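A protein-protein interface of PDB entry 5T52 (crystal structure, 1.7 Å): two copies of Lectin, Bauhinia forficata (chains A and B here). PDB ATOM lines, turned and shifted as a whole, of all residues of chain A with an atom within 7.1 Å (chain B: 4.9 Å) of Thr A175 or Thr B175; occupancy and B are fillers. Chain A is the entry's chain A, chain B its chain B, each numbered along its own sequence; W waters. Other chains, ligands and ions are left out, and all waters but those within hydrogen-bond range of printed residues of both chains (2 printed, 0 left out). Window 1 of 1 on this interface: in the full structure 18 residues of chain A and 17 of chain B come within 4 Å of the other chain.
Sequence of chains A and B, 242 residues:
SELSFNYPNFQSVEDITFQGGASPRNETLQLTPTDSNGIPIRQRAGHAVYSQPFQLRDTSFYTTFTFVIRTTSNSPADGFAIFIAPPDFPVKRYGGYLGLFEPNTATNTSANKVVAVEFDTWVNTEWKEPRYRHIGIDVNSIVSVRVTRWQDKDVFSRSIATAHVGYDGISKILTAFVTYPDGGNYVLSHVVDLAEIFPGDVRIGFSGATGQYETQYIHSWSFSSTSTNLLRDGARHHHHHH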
ATOM      1  N   PHE A  61       7.142 -17.078  10.854  1.00  0.00           N
ATOM      2  CA  PHE A  61       8.526 -16.769  11.123  1.00  0.00           C
ATOM      3  C   PHE A  61       8.758 -15.488  11.851  1.00  0.00           C
ATOM      4  O   PHE A  61       7.898 -14.626  11.903  1.00  0.00           O
ATOM      5  CB  PHE A  61       9.408 -16.769   9.771  1.00  0.00           C
ATOM      6  CG  PHE A  61       9.166 -15.573   8.863  1.00  0.00           C
ATOM      7  CD1 PHE A  61       9.674 -14.370   9.100  1.00  0.00           C
ATOM      8  CD2 PHE A  61       8.476 -15.784   7.660  1.00  0.00           C
ATOM      9  CE1 PHE A  61       9.455 -13.236   8.204  1.00  0.00           C
ATOM     10  CE2 PHE A  61       8.297 -14.742   6.765  1.00  0.00           C
ATOM     11  CZ  PHE A  61       8.747 -13.472   7.060  1.00  0.00           C
ATOM     12  N   THR A  63      12.173 -12.820  12.409  1.00  0.00           N
ATOM     13  CA  THR A  63      13.519 -12.365  12.158  1.00  0.00           C
ATOM     14  C   THR A  63      13.812 -10.992  12.761  1.00  0.00           C
ATOM     15  O   THR A  63      12.974 -10.132  12.847  1.00  0.00           O
ATOM     16  CB  THR A  63      13.791 -12.480  10.637  1.00  0.00           C
ATOM     17  OG1 THR A  63      15.194 -12.369  10.382  1.00  0.00           O
ATOM     18  CG2 THR A  63      13.060 -11.417   9.832  1.00  0.00           C
ATOM     19  N   VAL A 117      10.385  -5.368   3.311  1.00  0.00           N
ATOM     20  CA  VAL A 117      10.288  -4.234   4.121  1.00  0.00           C
ATOM     21  C   VAL A 117      11.435  -3.339   3.753  1.00  0.00           C
ATOM     22  O   VAL A 117      12.569  -3.677   3.869  1.00  0.00           O
ATOM     23  CB  VAL A 117      10.403  -4.634   5.595  1.00  0.00           C
ATOM     24  CG1 VAL A 117      10.366  -3.419   6.518  1.00  0.00           C
ATOM     25  CG2 VAL A 117       9.272  -5.571   5.968  1.00  0.00           C
ATOM     26  N   ILE A 137       6.164  -1.464   3.486  1.00  0.00           N
ATOM     27  CA  ILE A 137       6.021  -2.874   3.114  1.00  0.00           C
ATOM     28  C   ILE A 137       5.667  -2.908   1.611  1.00  0.00           C
ATOM     29  O   ILE A 137       4.803  -2.187   1.151  1.00  0.00           O
ATOM     30  CB  ILE A 137       4.845  -3.540   3.906  1.00  0.00           C
ATOM     31  CG1 ILE A 137       5.324  -3.641   5.345  1.00  0.00           C
ATOM     32  CG2 ILE A 137       4.555  -4.956   3.340  1.00  0.00           C
ATOM     33  CD1 ILE A 137       4.206  -4.176   6.264  1.00  0.00           C
ATOM     34  N   HIS A 164      12.518  -5.770  13.654  1.00  0.00           N
ATOM     35  CA  HIS A 164      11.930  -7.060  13.928  1.00  0.00           C
ATOM     36  C   HIS A 164      10.861  -7.267  12.867  1.00  0.00           C
ATOM     37  O   HIS A 164       9.998  -6.420  12.698  1.00  0.00           O
ATOM     38  CB  HIS A 164      11.198  -7.108  15.293  1.00  0.00           C
ATOM     39  CG  HIS A 164      12.039  -6.653  16.454  1.00  0.00           C
ATOM     40  ND1 HIS A 164      12.797  -7.511  17.200  1.00  0.00           N
ATOM     41  CD2 HIS A 164      12.309  -5.429  16.923  1.00  0.00           C
ATOM     42  CE1 HIS A 164      13.470  -6.853  18.140  1.00  0.00           C
ATOM     43  NE2 HIS A 164      13.197  -5.561  17.968  1.00  0.00           N
ATOM     44  N   VAL A 165      10.916  -8.385  12.179  1.00  0.00           N
ATOM     45  CA  VAL A 165       9.925  -8.675  11.107  1.00  0.00           C
ATOM     46  C   VAL A 165       9.371 -10.010  11.406  1.00  0.00           C
ATOM     47  O   VAL A 165      10.118 -11.047  11.514  1.00  0.00           O
ATOM     48  CB  VAL A 165      10.561  -8.578   9.713  1.00  0.00           C
ATOM     49  CG1 VAL A 165       9.586  -8.900   8.602  1.00  0.00           C
ATOM     50  CG2 VAL A 165      11.155  -7.210   9.414  1.00  0.00           C
ATOM     51  N   GLY A 166       8.041 -10.068  11.472  1.00  0.00           N
ATOM     52  CA  GLY A 166       7.405 -11.316  11.720  1.00  0.00           C
ATOM     53  C   GLY A 166       6.255 -11.612  10.786  1.00  0.00           C
ATOM     54  O   GLY A 166       5.624 -10.745  10.237  1.00  0.00           O
ATOM     55  N   TYR A 167       6.004 -12.899  10.611  1.00  0.00           N
ATOM     56  CA  TYR A 167       4.894 -13.329   9.794  1.00  0.00           C
ATOM     57  C   TYR A 167       4.072 -14.363  10.522  1.00  0.00           C
ATOM     58  O   TYR A 167       4.594 -15.422  10.913  1.00  0.00           O
ATOM     59  CB  TYR A 167       5.351 -13.879   8.471  1.00  0.00           C
ATOM     60  CG  TYR A 167       4.226 -14.211   7.533  1.00  0.00           C
ATOM     61  CD1 TYR A 167       3.366 -13.232   7.037  1.00  0.00           C
ATOM     62  CD2 TYR A 167       3.923 -15.521   7.287  1.00  0.00           C
ATOM     63  CE1 TYR A 167       2.334 -13.597   6.151  1.00  0.00           C
ATOM     64  CE2 TYR A 167       2.899 -15.868   6.382  1.00  0.00           C
ATOM     65  CZ  TYR A 167       2.065 -14.895   5.902  1.00  0.00           C
ATOM     66  OH  TYR A 167       1.003 -15.188   5.005  1.00  0.00           O
ATOM     67  N   ASP A 168       2.804 -14.059  10.757  1.00  0.00           N
ATOM     68  CA  ASP A 168       1.856 -14.931  11.377  1.00  0.00           C
ATOM     69  C   ASP A 168       1.107 -15.758  10.307  1.00  0.00           C
ATOM     70  O   ASP A 168       0.374 -15.203   9.574  1.00  0.00           O
ATOM     71  CB  ASP A 168       0.829 -14.106  12.152  1.00  0.00           C
ATOM     72  CG  ASP A 168      -0.194 -14.992  12.911  1.00  0.00           C
ATOM     73  OD1 ASP A 168      -0.323 -16.224  12.614  1.00  0.00           O
ATOM     74  OD2 ASP A 168      -0.831 -14.558  13.898  1.00  0.00           O
ATOM     75  N   ILE A 173      -0.407 -12.245   8.255  1.00  0.00           N
ATOM     76  CA  ILE A 173      -0.080 -10.875   8.518  1.00  0.00           C
ATOM     77  C   ILE A 173       1.413 -10.720   8.733  1.00  0.00           C
ATOM     78  O   ILE A 173       2.028 -11.496   9.477  1.00  0.00           O
ATOM     79  CB  ILE A 173      -0.753 -10.307   9.785  1.00  0.00           C
ATOM     80  CG1 ILE A 173      -2.278 -10.212   9.597  1.00  0.00           C
ATOM     81  CG2 ILE A 173      -0.149  -8.975  10.225  1.00  0.00           C
ATOM     82  CD1 ILE A 173      -3.101  -9.981  10.838  1.00  0.00           C
ATOM     83  N   LEU A 174       1.999  -9.859   7.904  1.00  0.00           N
ATOM     84  CA  LEU A 174       3.413  -9.458   7.997  1.00  0.00           C
ATOM     85  C   LEU A 174       3.518  -8.162   8.783  1.00  0.00           C
ATOM     86  O   LEU A 174       2.888  -7.179   8.493  1.00  0.00           O
ATOM     87  CB  LEU A 174       3.949  -9.286   6.510  1.00  0.00           C
ATOM     88  CG  LEU A 174       5.457  -8.886   6.460  1.00  0.00           C
ATOM     89  CD1 LEU A 174       6.368 -10.035   6.823  1.00  0.00           C
ATOM     90  CD2 LEU A 174       5.768  -8.472   5.025  1.00  0.00           C
ATOM     91  N   THR A 175       4.404  -8.139   9.780  1.00  0.00           N
ATOM     92  CA  THR A 175       4.558  -6.983  10.607  1.00  0.00           C
ATOM     93  C   THR A 175       6.040  -6.652  10.755  1.00  0.00           C
ATOM     94  O   THR A 175       6.896  -7.522  10.865  1.00  0.00           O
ATOM     95  CB  THR A 175       4.064  -7.318  12.025  1.00  0.00           C
ATOM     96  OG1 THR A 175       2.663  -7.555  11.950  1.00  0.00           O
ATOM     97  CG2 THR A 175       4.335  -6.225  13.027  1.00  0.00           C
ATOM     98  N   ALA A 176       6.328  -5.374  10.697  1.00  0.00           N
ATOM     99  CA  ALA A 176       7.648  -4.847  11.069  1.00  0.00           C
ATOM    100  C   ALA A 176       7.572  -3.918  12.230  1.00  0.00           C
ATOM    101  O   ALA A 176       6.778  -2.926  12.207  1.00  0.00           O
ATOM    102  CB  ALA A 176       8.229  -4.144   9.899  1.00  0.00           C
ATOM    103  N   PHE A 177       8.501  -4.054  13.162  1.00  0.00           N
ATOM    104  CA  PHE A 177       8.757  -3.072  14.181  1.00  0.00           C
ATOM    105  C   PHE A 177      10.205  -2.629  14.005  1.00  0.00           C
ATOM    106  O   PHE A 177      11.087  -3.466  13.952  1.00  0.00           O
ATOM    107  CB  PHE A 177       8.664  -3.611  15.601  1.00  0.00           C
ATOM    108  CG  PHE A 177       7.341  -4.278  15.967  1.00  0.00           C
ATOM    109  CD1 PHE A 177       6.113  -3.871  15.452  1.00  0.00           C
ATOM    110  CD2 PHE A 177       7.329  -5.356  16.921  1.00  0.00           C
ATOM    111  CE1 PHE A 177       4.910  -4.427  15.900  1.00  0.00           C
ATOM    112  CE2 PHE A 177       6.151  -5.914  17.354  1.00  0.00           C
ATOM    113  CZ  PHE A 177       4.924  -5.487  16.834  1.00  0.00           C
ATOM    114  N   VAL A 187       5.938   1.064  13.447  1.00  0.00           N
ATOM    115  CA  VAL A 187       5.145  -0.123  13.369  1.00  0.00           C
ATOM    116  C   VAL A 187       4.358  -0.160  12.019  1.00  0.00           C
ATOM    117  O   VAL A 187       3.586   0.779  11.686  1.00  0.00           O
ATOM    118  CB  VAL A 187       4.155  -0.193  14.526  1.00  0.00           C
ATOM    119  CG1 VAL A 187       3.183  -1.300  14.339  1.00  0.00           C
ATOM    120  CG2 VAL A 187       4.866  -0.183  15.853  1.00  0.00           C
ATOM    121  N   LEU A 188       4.496  -1.260  11.299  1.00  0.00           N
ATOM    122  CA  LEU A 188       3.660  -1.491  10.081  1.00  0.00           C
ATOM    123  C   LEU A 188       3.212  -2.883  10.001  1.00  0.00           C
ATOM    124  O   LEU A 188       4.042  -3.808  10.131  1.00  0.00           O
ATOM    125  CB  LEU A 188       4.499  -1.247   8.773  1.00  0.00           C
ATOM    126  CG  LEU A 188       4.911   0.193   8.488  1.00  0.00           C
ATOM    127  CD1 LEU A 188       5.572   0.287   7.106  1.00  0.00           C
ATOM    128  CD2 LEU A 188       3.669   0.961   8.383  1.00  0.00           C
ATOM    129  N   SER A 189       1.949  -3.127   9.689  1.00  0.00           N
ATOM    130  CA  SER A 189       1.504  -4.503   9.549  1.00  0.00           C
ATOM    131  C   SER A 189       0.584  -4.546   8.348  1.00  0.00           C
ATOM    132  O   SER A 189      -0.199  -3.579   8.121  1.00  0.00           O
ATOM    133  CB  SER A 189       0.655  -4.922  10.771  1.00  0.00           C
ATOM    134  OG  SER A 189       1.364  -5.027  12.001  1.00  0.00           O
ATOM    135  N   HIS A 190       0.609  -5.641   7.663  1.00  0.00           N
ATOM    136  CA  HIS A 190      -0.179  -5.791   6.452  1.00  0.00           C
ATOM    137  C   HIS A 190      -0.581  -7.234   6.245  1.00  0.00           C
ATOM    138  O   HIS A 190       0.231  -8.128   6.380  1.00  0.00           O
ATOM    139  CB  HIS A 190       0.681  -5.321   5.296  1.00  0.00           C
ATOM    140  CG  HIS A 190      -0.019  -5.335   3.962  1.00  0.00           C
ATOM    141  ND1 HIS A 190      -1.064  -4.505   3.641  1.00  0.00           N
ATOM    142  CD2 HIS A 190       0.196  -6.103   2.878  1.00  0.00           C
ATOM    143  CE1 HIS A 190      -1.448  -4.728   2.381  1.00  0.00           C
ATOM    144  NE2 HIS A 190      -0.707  -5.725   1.900  1.00  0.00           N
ATOM    145  N   HIS B 164       7.450  -7.832  22.498  1.00  0.00           N
ATOM    146  CA  HIS B 164       7.224  -6.651  21.758  1.00  0.00           C
ATOM    147  C   HIS B 164       5.753  -6.635  21.348  1.00  0.00           C
ATOM    148  O   HIS B 164       5.280  -7.600  20.725  1.00  0.00           O
ATOM    149  CB  HIS B 164       8.094  -6.730  20.452  1.00  0.00           C
ATOM    150  CG  HIS B 164       9.542  -6.893  20.674  1.00  0.00           C
ATOM    151  ND1 HIS B 164      10.408  -5.838  20.801  1.00  0.00           N
ATOM    152  CD2 HIS B 164      10.290  -8.018  20.767  1.00  0.00           C
ATOM    153  CE1 HIS B 164      11.621  -6.291  21.015  1.00  0.00           C
ATOM    154  NE2 HIS B 164      11.580  -7.621  20.967  1.00  0.00           N
ATOM    155  N   VAL B 165       5.003  -5.555  21.616  1.00  0.00           N
ATOM    156  CA  VAL B 165       3.638  -5.506  21.234  1.00  0.00           C
ATOM    157  C   VAL B 165       3.379  -4.233  20.526  1.00  0.00           C
ATOM    158  O   VAL B 165       3.702  -3.159  20.962  1.00  0.00           O
ATOM    159  CB  VAL B 165       2.647  -5.665  22.468  1.00  0.00           C
ATOM    160  CG1 VAL B 165       1.193  -5.499  22.102  1.00  0.00           C
ATOM    161  CG2 VAL B 165       2.976  -7.000  23.231  1.00  0.00           C
ATOM    162  N   GLY B 166       2.821  -4.326  19.324  1.00  0.00           N
ATOM    163  CA  GLY B 166       2.591  -3.155  18.547  1.00  0.00           C
ATOM    164  C   GLY B 166       1.195  -3.147  17.938  1.00  0.00           C
ATOM    165  O   GLY B 166       0.563  -4.218  17.750  1.00  0.00           O
ATOM    166  N   ILE B 173      -4.231  -3.678  13.210  1.00  0.00           N
ATOM    167  CA  ILE B 173      -3.641  -5.009  13.559  1.00  0.00           C
ATOM    168  C   ILE B 173      -2.803  -4.879  14.833  1.00  0.00           C
ATOM    169  O   ILE B 173      -1.953  -3.995  14.917  1.00  0.00           O
ATOM    170  CB  ILE B 173      -2.720  -5.453  12.431  1.00  0.00           C
ATOM    171  CG1 ILE B 173      -3.658  -5.758  11.239  1.00  0.00           C
ATOM    172  CG2 ILE B 173      -1.946  -6.694  12.863  1.00  0.00           C
ATOM    173  CD1 ILE B 173      -2.932  -5.922   9.930  1.00  0.00           C
ATOM    174  N   LEU B 174      -3.096  -5.727  15.792  1.00  0.00           N
ATOM    175  CA  LEU B 174      -2.348  -5.885  17.033  1.00  0.00           C
ATOM    176  C   LEU B 174      -1.418  -7.096  16.897  1.00  0.00           C
ATOM    177  O   LEU B 174      -1.837  -8.190  16.503  1.00  0.00           O
ATOM    178  CB  LEU B 174      -3.279  -6.146  18.234  1.00  0.00           C
ATOM    179  CG  LEU B 174      -2.588  -6.229  19.575  1.00  0.00           C
ATOM    180  CD1 LEU B 174      -2.024  -4.914  19.988  1.00  0.00           C
ATOM    181  CD2 LEU B 174      -3.602  -6.795  20.586  1.00  0.00           C
ATOM    182  N   THR B 175      -0.116  -6.855  17.166  1.00  0.00           N
ATOM    183  CA  THR B 175       0.884  -7.892  17.009  1.00  0.00           C
ATOM    184  C   THR B 175       1.698  -8.086  18.255  1.00  0.00           C
ATOM    185  O   THR B 175       2.144  -7.090  18.827  1.00  0.00           O
ATOM    186  CB  THR B 175       1.830  -7.547  15.816  1.00  0.00           C
ATOM    187  OG1 THR B 175       1.069  -7.674  14.622  1.00  0.00           O
ATOM    188  CG2 THR B 175       2.950  -8.627  15.759  1.00  0.00           C
ATOM    189  N   ALA B 176       2.034  -9.363  18.563  1.00  0.00           N
ATOM    190  CA  ALA B 176       2.978  -9.610  19.620  1.00  0.00           C
ATOM    191  C   ALA B 176       4.076 -10.487  19.114  1.00  0.00           C
ATOM    192  O   ALA B 176       3.810 -11.464  18.457  1.00  0.00           O
ATOM    193  CB  ALA B 176       2.303 -10.291  20.775  1.00  0.00           C
ATOM    194  N   PHE B 177       5.300 -10.092  19.411  1.00  0.00           N
ATOM    195  CA  PHE B 177       6.454 -10.954  19.185  1.00  0.00           C
ATOM    196  C   PHE B 177       7.029 -11.248  20.552  1.00  0.00           C
ATOM    197  O   PHE B 177       7.260 -10.363  21.318  1.00  0.00           O
ATOM    198  CB  PHE B 177       7.615 -10.321  18.362  1.00  0.00           C
ATOM    199  CG  PHE B 177       7.300  -9.846  16.930  1.00  0.00           C
ATOM    200  CD1 PHE B 177       6.268 -10.369  16.218  1.00  0.00           C
ATOM    201  CD2 PHE B 177       7.994  -8.770  16.384  1.00  0.00           C
ATOM    202  CE1 PHE B 177       6.058 -10.002  14.900  1.00  0.00           C
ATOM    203  CE2 PHE B 177       7.792  -8.342  15.080  1.00  0.00           C
ATOM    204  CZ  PHE B 177       6.774  -8.919  14.344  1.00  0.00           C
ATOM    205  N   LEU B 188       2.191 -13.582  17.057  1.00  0.00           N
ATOM    206  CA  LEU B 188       0.784 -13.572  16.926  1.00  0.00           C
ATOM    207  C   LEU B 188       0.300 -12.234  16.458  1.00  0.00           C
ATOM    208  O   LEU B 188       0.652 -11.222  17.024  1.00  0.00           O
ATOM    209  CB  LEU B 188       0.051 -13.788  18.280  1.00  0.00           C
ATOM    210  CG  LEU B 188       0.306 -15.027  19.047  1.00  0.00           C
ATOM    211  CD1 LEU B 188      -0.537 -14.955  20.331  1.00  0.00           C
ATOM    212  CD2 LEU B 188      -0.028 -16.256  18.264  1.00  0.00           C
ATOM    213  N   SER B 189      -0.563 -12.219  15.430  1.00  0.00           N
ATOM    214  CA  SER B 189      -1.156 -10.990  14.967  1.00  0.00           C
ATOM    215  C   SER B 189      -2.685 -11.158  14.820  1.00  0.00           C
ATOM    216  O   SER B 189      -3.157 -12.239  14.469  1.00  0.00           O
ATOM    217  CB  SER B 189      -0.616 -10.559  13.648  1.00  0.00           C
ATOM    218  OG  SER B 189       0.796 -10.201  13.705  1.00  0.00           O
HETATM  219  O   HOH W   1       0.831  -4.793  14.536  1.00  0.00           O
HETATM  220  O   HOH W   2       2.910 -10.392  12.028  1.00  0.00           O
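OD2 of Asp A168 sits at hydrogen-bond distance from N of Ser B189. OG1 of Thr A175 sits at hydrogen-bond distance from OG1 of Thr B175.
The backbone NH (N) of Ala B176 sits at hydrogen-bond distance from the backbone carbonyl oxygen (O) of Leu B188 (2.8 Å). The backbone NH of His A164 is in hydrogen-bond range of the backbone carbonyl oxygen of Phe A177 (2.7 Å). The side-chain hydroxyl (OG1) of Thr A175 lies within hydrogen-bond range of the side-chain hydroxyl (OG) of Ser A189, at 2.8 Å. The backbone carbonyl oxygen (O) of Ile A173 sits at hydrogen-bond distance from the backbone NH (N) of Asp A168 (3.0 Å). OG1 of Thr B175 lies within hydrogen-bond range of OG of Ser B189, at 2.7 Å. O of Phe B177 sits at hydrogen-bond distance from N of His B164, at 2.8 Å.
Among the printed residues, pairs that only touch across the chains: Gly A166 with Phe B177 (3.3 Å), Phe A177 with Gly B166 (3.5 Å), His A164 with His B164 (3.5 Å), Phe A177 with Phe B177 (3.5 Å), Asp A168 with Leu B188 (3.6 Å), His A164 with Phe B177 (3.6 Å), Thr A175 with Ser B189 (3.7 Å), Ser A189 with Thr B175 (3.7 Å), Phe A177 with His B164 (3.7 Å), Thr A175 with Phe B177 (3.8 Å), Phe A177 with Thr B175 (3.8 Å), Ser A189 with Ile B173 (3.8 Å), Ile A173 with Ser B189 (3.8 Å) and Ile A173 with Ile B173 (3.9 Å).
Of chain B, only Thr B175, Phe B177 and Ser B189 come within 4 Å of Thr A175. Of the printed residues of chain A, Thr B175 touches Thr A175 (3.1 Å), Phe A177 (3.8 Å) and Ser A189 (3.7 Å). Printed residues of chain B within 4 Å of Phe A177: His B164 (3.7 Å), Gly B166 (3.5 Å), Thr B175 (3.8 Å) and Phe B177 (3.5 Å). Of the printed residues of chain A, Phe B177 touches His A164 (3.6 Å), Gly A166 (3.3 Å), Thr A175 (3.8 Å) and Phe A177 (3.5 Å). Of the printed residues of chain A, Leu B188 touches Asp A168. Of the printed residues of chain B, His A164 touches His B164 (3.5 Å) and Phe B177 (3.6 Å). Of the printed residues of chain B, Asp A168 touches Leu B188 and Ser B189. Tyr A167 touches none of the printed residues of chain B. Ala B176 touches none of the printed residues of chain A. The nearest residue of chain A that does not touch Thr B175 is Ile A173 (4.7 Å). The nearest printed residue of chain A that does not touch Ile B173 is His A190 (4.2 Å).
Along chain B the printed residues that touch a printed residue of chain A span positions 164 to 189. Of the 18 printed residues of chain A, 7 touch a printed residue of chain B.
Thr B175 touches its own counterpart, Thr A175. Thr A175 touches Phe B177, and with the chains exchanged Phe A177 touches Thr B175. Thr A175 touches Ser B189, and with the chains exchanged Ser A189 touches Thr B175. Phe A177 touches its own counterpart, Phe B177. Positions printed for both chains: 164, 165, 166, 173, 174, 175, 176, 177, 188 and 189. Of the 16 pairs that touch across the chains among the printed residues, 14 have their exchanged pair printed and touching as well.
Water W1 lies within hydrogen-bond range of the side-chain hydroxyl of Ser A189 (2.6 Å), the side-chain hydroxyl of Thr B175 (2.9 Å), the backbone carbonyl oxygen of Ile B173 (2.9 Å) and the backbone carbonyl oxygen of Gly B166 (3.3 Å). Water W2 lies within hydrogen-bond range of the side-chain hydroxyl (OG) of Ser B189 (2.7 Å), the side-chain hydroxyl (OG1) of Thr A175 (2.8 Å), the backbone carbonyl oxygen (O) of Ile A173 (2.9 Å) and the backbone carbonyl oxygen (O) of Gly A166 (3.3 Å).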
